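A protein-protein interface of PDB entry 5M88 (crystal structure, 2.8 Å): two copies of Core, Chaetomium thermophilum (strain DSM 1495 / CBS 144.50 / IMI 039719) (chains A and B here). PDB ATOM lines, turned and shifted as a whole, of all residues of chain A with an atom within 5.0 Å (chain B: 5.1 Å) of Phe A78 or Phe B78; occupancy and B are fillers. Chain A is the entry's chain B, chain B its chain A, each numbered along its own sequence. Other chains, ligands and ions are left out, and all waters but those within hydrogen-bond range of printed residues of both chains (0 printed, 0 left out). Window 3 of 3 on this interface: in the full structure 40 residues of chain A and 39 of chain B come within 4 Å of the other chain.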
ATOM      1  N   LEU A  74       3.962  -8.696   8.426  1.00  0.00           N
ATOM      2  CA  LEU A  74       4.512  -9.936   7.890  1.00  0.00           C
ATOM      3  C   LEU A  74       3.953 -10.233   6.506  1.00  0.00           C
ATOM      4  O   LEU A  74       4.690 -10.654   5.605  1.00  0.00           O
ATOM      5  CB  LEU A  74       4.209 -11.089   8.847  1.00  0.00           C
ATOM      6  CG  LEU A  74       5.324 -12.094   9.109  1.00  0.00           C
ATOM      7  CD1 LEU A  74       6.537 -11.393   9.690  1.00  0.00           C
ATOM      8  CD2 LEU A  74       4.831 -13.185  10.044  1.00  0.00           C
ATOM      9  N   LEU A  75       2.650 -10.012   6.317  1.00  0.00           N
ATOM     10  CA  LEU A  75       2.056 -10.162   4.993  1.00  0.00           C
ATOM     11  C   LEU A  75       2.612  -9.131   4.020  1.00  0.00           C
ATOM     12  O   LEU A  75       2.844  -9.442   2.848  1.00  0.00           O
ATOM     13  CB  LEU A  75       0.535 -10.058   5.081  1.00  0.00           C
ATOM     14  CG  LEU A  75      -0.154 -11.061   6.008  1.00  0.00           C
ATOM     15  CD1 LEU A  75      -1.651 -10.813   6.043  1.00  0.00           C
ATOM     16  CD2 LEU A  75       0.149 -12.486   5.582  1.00  0.00           C
ATOM     17  N   LYS A  76       2.837  -7.901   4.487  1.00  0.00           N
ATOM     18  CA  LYS A  76       3.451  -6.896   3.626  1.00  0.00           C
ATOM     19  C   LYS A  76       4.847  -7.329   3.189  1.00  0.00           C
ATOM     20  O   LYS A  76       5.228  -7.145   2.027  1.00  0.00           O
ATOM     21  CB  LYS A  76       3.502  -5.549   4.349  1.00  0.00           C
ATOM     22  CG  LYS A  76       4.055  -4.404   3.512  1.00  0.00           C
ATOM     23  CD  LYS A  76       3.078  -3.987   2.425  1.00  0.00           C
ATOM     24  CE  LYS A  76       3.494  -2.670   1.785  1.00  0.00           C
ATOM     25  NZ  LYS A  76       4.834  -2.763   1.143  1.00  0.00           N
ATOM     26  N   ALA A  77       5.618  -7.919   4.106  1.00  0.00           N
ATOM     27  CA  ALA A  77       6.957  -8.396   3.766  1.00  0.00           C
ATOM     28  C   ALA A  77       6.904  -9.553   2.773  1.00  0.00           C
ATOM     29  O   ALA A  77       7.702  -9.603   1.828  1.00  0.00           O
ATOM     30  CB  ALA A  77       7.699  -8.810   5.036  1.00  0.00           C
ATOM     31  N   PHE A  78       5.988 -10.502   2.986  1.00  0.00           N
ATOM     32  CA  PHE A  78       5.779 -11.570   2.011  1.00  0.00           C
ATOM     33  C   PHE A  78       5.461 -10.997   0.634  1.00  0.00           C
ATOM     34  O   PHE A  78       6.003 -11.446  -0.384  1.00  0.00           O
ATOM     35  CB  PHE A  78       4.646 -12.490   2.468  1.00  0.00           C
ATOM     36  CG  PHE A  78       5.013 -13.407   3.596  1.00  0.00           C
ATOM     37  CD1 PHE A  78       6.237 -14.051   3.617  1.00  0.00           C
ATOM     38  CD2 PHE A  78       4.122 -13.632   4.635  1.00  0.00           C
ATOM     39  CE1 PHE A  78       6.570 -14.904   4.657  1.00  0.00           C
ATOM     40  CE2 PHE A  78       4.450 -14.479   5.677  1.00  0.00           C
ATOM     41  CZ  PHE A  78       5.677 -15.116   5.690  1.00  0.00           C
ATOM     42  N   GLN A  79       4.570 -10.002   0.588  1.00  0.00           N
ATOM     43  CA  GLN A  79       4.179  -9.404  -0.684  1.00  0.00           C
ATOM     44  C   GLN A  79       5.359  -8.717  -1.355  1.00  0.00           C
ATOM     45  O   GLN A  79       5.538  -8.823  -2.575  1.00  0.00           O
ATOM     46  CB  GLN A  79       3.040  -8.409  -0.458  1.00  0.00           C
ATOM     47  CG  GLN A  79       2.391  -7.897  -1.731  1.00  0.00           C
ATOM     48  CD  GLN A  79       1.607  -8.974  -2.448  1.00  0.00           C
ATOM     49  OE1 GLN A  79       2.145  -9.696  -3.289  1.00  0.00           O
ATOM     50  NE2 GLN A  79       0.326  -9.093  -2.116  1.00  0.00           N
ATOM     51  N   ASP A  80       6.181  -8.017  -0.574  1.00  0.00           N
ATOM     52  CA  ASP A  80       7.345  -7.348  -1.144  1.00  0.00           C
ATOM     53  C   ASP A  80       8.347  -8.357  -1.691  1.00  0.00           C
ATOM     54  O   ASP A  80       8.919  -8.152  -2.769  1.00  0.00           O
ATOM     55  CB  ASP A  80       7.996  -6.447  -0.095  1.00  0.00           C
ATOM     56  CG  ASP A  80       7.100  -5.294   0.314  1.00  0.00           C
ATOM     57  OD1 ASP A  80       6.226  -4.906  -0.490  1.00  0.00           O
ATOM     58  OD2 ASP A  80       7.271  -4.771   1.436  1.00  0.00           O
ATOM     59  N   GLU A  81       8.560  -9.459  -0.971  1.00  0.00           N
ATOM     60  CA  GLU A  81       9.483 -10.481  -1.455  1.00  0.00           C
ATOM     61  C   GLU A  81       8.965 -11.134  -2.731  1.00  0.00           C
ATOM     62  O   GLU A  81       9.741 -11.399  -3.660  1.00  0.00           O
ATOM     63  CB  GLU A  81       9.715 -11.530  -0.367  1.00  0.00           C
ATOM     64  CG  GLU A  81      10.931 -12.416  -0.595  1.00  0.00           C
ATOM     65  CD  GLU A  81      12.241 -11.664  -0.438  1.00  0.00           C
ATOM     66  OE1 GLU A  81      12.233 -10.561   0.150  1.00  0.00           O
ATOM     67  OE2 GLU A  81      13.282 -12.182  -0.895  1.00  0.00           O
ATOM     68  N   TRP A  82       7.656 -11.391  -2.798  1.00  0.00           N
ATOM     69  CA  TRP A  82       7.079 -11.961  -4.012  1.00  0.00           C
ATOM     70  C   TRP A  82       7.211 -11.002  -5.186  1.00  0.00           C
ATOM     71  O   TRP A  82       7.535 -11.419  -6.306  1.00  0.00           O
ATOM     72  CB  TRP A  82       5.615 -12.324  -3.777  1.00  0.00           C
ATOM     73  CG  TRP A  82       4.967 -12.996  -4.943  1.00  0.00           C
ATOM     74  CD1 TRP A  82       4.942 -14.332  -5.205  1.00  0.00           C
ATOM     75  CD2 TRP A  82       4.227 -12.368  -5.997  1.00  0.00           C
ATOM     76  NE1 TRP A  82       4.236 -14.579  -6.358  1.00  0.00           N
ATOM     77  CE2 TRP A  82       3.788 -13.388  -6.865  1.00  0.00           C
ATOM     78  CE3 TRP A  82       3.893 -11.041  -6.292  1.00  0.00           C
ATOM     79  CZ2 TRP A  82       3.040 -13.124  -8.011  1.00  0.00           C
ATOM     80  CZ3 TRP A  82       3.151 -10.781  -7.428  1.00  0.00           C
ATOM     81  CH2 TRP A  82       2.732 -11.818  -8.275  1.00  0.00           C
ATOM     82  N   ASP A  83       6.961  -9.710  -4.950  1.00  0.00           N
ATOM     83  CA  ASP A  83       7.144  -8.716  -6.002  1.00  0.00           C
ATOM     84  C   ASP A  83       8.587  -8.695  -6.490  1.00  0.00           C
ATOM     85  O   ASP A  83       8.843  -8.644  -7.700  1.00  0.00           O
ATOM     86  CB  ASP A  83       6.738  -7.331  -5.494  1.00  0.00           C
ATOM     87  CG  ASP A  83       5.253  -7.227  -5.194  1.00  0.00           C
ATOM     88  OD1 ASP A  83       4.483  -8.084  -5.674  1.00  0.00           O
ATOM     89  OD2 ASP A  83       4.854  -6.274  -4.489  1.00  0.00           O
ATOM     90  N   LEU B  74      -1.928 -24.046   4.089  1.00  0.00           N
ATOM     91  CA  LEU B  74      -1.840 -22.801   3.333  1.00  0.00           C
ATOM     92  C   LEU B  74      -0.423 -22.240   3.380  1.00  0.00           C
ATOM     93  O   LEU B  74       0.094 -21.733   2.371  1.00  0.00           O
ATOM     94  CB  LEU B  74      -2.850 -21.800   3.882  1.00  0.00           C
ATOM     95  CG  LEU B  74      -3.654 -21.025   2.842  1.00  0.00           C
ATOM     96  CD1 LEU B  74      -4.419 -21.998   1.963  1.00  0.00           C
ATOM     97  CD2 LEU B  74      -4.616 -20.077   3.534  1.00  0.00           C
ATOM     98  N   LEU B  75       0.225 -22.334   4.546  1.00  0.00           N
ATOM     99  CA  LEU B  75       1.627 -21.947   4.655  1.00  0.00           C
ATOM    100  C   LEU B  75       2.507 -22.841   3.791  1.00  0.00           C
ATOM    101  O   LEU B  75       3.462 -22.370   3.163  1.00  0.00           O
ATOM    102  CB  LEU B  75       2.073 -22.015   6.115  1.00  0.00           C
ATOM    103  CG  LEU B  75       1.295 -21.172   7.129  1.00  0.00           C
ATOM    104  CD1 LEU B  75       1.826 -21.407   8.530  1.00  0.00           C
ATOM    105  CD2 LEU B  75       1.364 -19.692   6.770  1.00  0.00           C
ATOM    106  N   LYS B  76       2.189 -24.138   3.743  1.00  0.00           N
ATOM    107  CA  LYS B  76       2.920 -25.067   2.885  1.00  0.00           C
ATOM    108  C   LYS B  76       2.783 -24.680   1.418  1.00  0.00           C
ATOM    109  O   LYS B  76       3.753 -24.757   0.656  1.00  0.00           O
ATOM    110  CB  LYS B  76       2.415 -26.491   3.119  1.00  0.00           C
ATOM    111  CG  LYS B  76       3.147 -27.582   2.348  1.00  0.00           C
ATOM    112  CD  LYS B  76       4.546 -27.815   2.900  1.00  0.00           C
ATOM    113  CE  LYS B  76       5.160 -29.096   2.351  1.00  0.00           C
ATOM    114  NZ  LYS B  76       5.305 -29.085   0.866  1.00  0.00           N
ATOM    115  N   ALA B  77       1.585 -24.262   1.006  1.00  0.00           N
ATOM    116  CA  ALA B  77       1.375 -23.842  -0.377  1.00  0.00           C
ATOM    117  C   ALA B  77       2.156 -22.573  -0.699  1.00  0.00           C
ATOM    118  O   ALA B  77       2.761 -22.461  -1.775  1.00  0.00           O
ATOM    119  CB  ALA B  77      -0.116 -23.630  -0.636  1.00  0.00           C
ATOM    120  N   PHE B  78       2.135 -21.598   0.214  1.00  0.00           N
ATOM    121  CA  PHE B  78       2.958 -20.405   0.037  1.00  0.00           C
ATOM    122  C   PHE B  78       4.427 -20.776  -0.127  1.00  0.00           C
ATOM    123  O   PHE B  78       5.115 -20.271  -1.024  1.00  0.00           O
ATOM    124  CB  PHE B  78       2.770 -19.453   1.219  1.00  0.00           C
ATOM    125  CG  PHE B  78       3.550 -18.178   1.094  1.00  0.00           C
ATOM    126  CD1 PHE B  78       3.009 -17.082   0.439  1.00  0.00           C
ATOM    127  CD2 PHE B  78       4.825 -18.072   1.628  1.00  0.00           C
ATOM    128  CE1 PHE B  78       3.728 -15.908   0.316  1.00  0.00           C
ATOM    129  CE2 PHE B  78       5.548 -16.900   1.507  1.00  0.00           C
ATOM    130  CZ  PHE B  78       4.998 -15.816   0.849  1.00  0.00           C
ATOM    131  N   GLN B  79       4.920 -21.670   0.733  1.00  0.00           N
ATOM    132  CA  GLN B  79       6.321 -22.074   0.663  1.00  0.00           C
ATOM    133  C   GLN B  79       6.630 -22.792  -0.647  1.00  0.00           C
ATOM    134  O   GLN B  79       7.705 -22.605  -1.227  1.00  0.00           O
ATOM    135  CB  GLN B  79       6.670 -22.956   1.859  1.00  0.00           C
ATOM    136  CG  GLN B  79       8.154 -23.238   2.014  1.00  0.00           C
ATOM    137  CD  GLN B  79       8.440 -24.192   3.160  1.00  0.00           C
ATOM    138  OE1 GLN B  79       7.746 -25.195   3.337  1.00  0.00           O
ATOM    139  NE2 GLN B  79       9.460 -23.877   3.952  1.00  0.00           N
ATOM    140  N   ASP B  80       5.704 -23.628  -1.124  1.00  0.00           N
ATOM    141  CA  ASP B  80       5.931 -24.331  -2.382  1.00  0.00           C
ATOM    142  C   ASP B  80       6.008 -23.359  -3.549  1.00  0.00           C
ATOM    143  O   ASP B  80       6.874 -23.491  -4.423  1.00  0.00           O
ATOM    144  CB  ASP B  80       4.829 -25.364  -2.618  1.00  0.00           C
ATOM    145  CG  ASP B  80       4.857 -26.489  -1.600  1.00  0.00           C
ATOM    146  OD1 ASP B  80       5.936 -26.744  -1.022  1.00  0.00           O
ATOM    147  OD2 ASP B  80       3.802 -27.124  -1.382  1.00  0.00           O
ATOM    148  N   GLU B  81       5.125 -22.359  -3.570  1.00  0.00           N
ATOM    149  CA  GLU B  81       5.181 -21.369  -4.642  1.00  0.00           C
ATOM    150  C   GLU B  81       6.469 -20.556  -4.569  1.00  0.00           C
ATOM    151  O   GLU B  81       7.072 -20.231  -5.601  1.00  0.00           O
ATOM    152  CB  GLU B  81       3.957 -20.457  -4.583  1.00  0.00           C
ATOM    153  CG  GLU B  81       3.700 -19.677  -5.867  1.00  0.00           C
ATOM    154  CD  GLU B  81       3.232 -20.566  -7.004  1.00  0.00           C
ATOM    155  OE1 GLU B  81       2.790 -21.703  -6.729  1.00  0.00           O
ATOM    156  OE2 GLU B  81       3.304 -20.128  -8.171  1.00  0.00           O
ATOM    157  N   TRP B  82       6.911 -20.225  -3.354  1.00  0.00           N
ATOM    158  CA  TRP B  82       8.169 -19.502  -3.201  1.00  0.00           C
ATOM    159  C   TRP B  82       9.344 -20.330  -3.713  1.00  0.00           C
ATOM    160  O   TRP B  82      10.230 -19.806  -4.402  1.00  0.00           O
ATOM    161  CB  TRP B  82       8.372 -19.130  -1.734  1.00  0.00           C
ATOM    162  CG  TRP B  82       9.588 -18.303  -1.483  1.00  0.00           C
ATOM    163  CD1 TRP B  82       9.674 -16.940  -1.507  1.00  0.00           C
ATOM    164  CD2 TRP B  82      10.901 -18.783  -1.169  1.00  0.00           C
ATOM    165  NE1 TRP B  82      10.959 -16.542  -1.220  1.00  0.00           N
ATOM    166  CE2 TRP B  82      11.732 -17.655  -1.012  1.00  0.00           C
ATOM    167  CE3 TRP B  82      11.455 -20.059  -1.005  1.00  0.00           C
ATOM    168  CZ2 TRP B  82      13.090 -17.765  -0.700  1.00  0.00           C
ATOM    169  CZ3 TRP B  82      12.802 -20.167  -0.696  1.00  0.00           C
ATOM    170  CH2 TRP B  82      13.605 -19.025  -0.549  1.00  0.00           C
ATOM    171  N   ASP B  83       9.360 -21.629  -3.391  1.00  0.00           N
ATOM    172  CA  ASP B  83      10.405 -22.512  -3.902  1.00  0.00           C
ATOM    173  C   ASP B  83      10.393 -22.553  -5.424  1.00  0.00           C
ATOM    174  O   ASP B  83      11.452 -22.514  -6.064  1.00  0.00           O
ATOM    175  CB  ASP B  83      10.240 -23.925  -3.337  1.00  0.00           C
ATOM    176  CG  ASP B  83      10.484 -23.997  -1.838  1.00  0.00           C
ATOM    177  OD1 ASP B  83      11.100 -23.067  -1.276  1.00  0.00           O
ATOM    178  OD2 ASP B  83      10.071 -25.002  -1.220  1.00  0.00           O
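Phe B78 touches Phe A78.
Ala A77 touches none of the printed residues of chain B.
Lys B76 touches none of the printed residues of chain A.
Phe B78 touches just one residue of chain A: Phe A78 (3.5 Å).
Of the 10 printed residues of chain A, 1 touches a printed residue of chain B.
Printed residues of chain A that touch a printed residue of chain B: Phe A78.
Hydrophobic or aromatic side chains of chain A that line the printed part of chain B: Phe A78.
Hydrophobic or aromatic side chains of chain B within 4 Å of the printed part of chain A: Phe B78.
Among the printed residues, 1 pair touches across the chains.
Among the printed residues, no Asp or Glu carboxylate lies within 4 Å of a Lys or Arg side-chain nitrogen of the other chain.
Phe A78 touches its own counterpart, Phe B78.
10 positions are printed for both chains.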
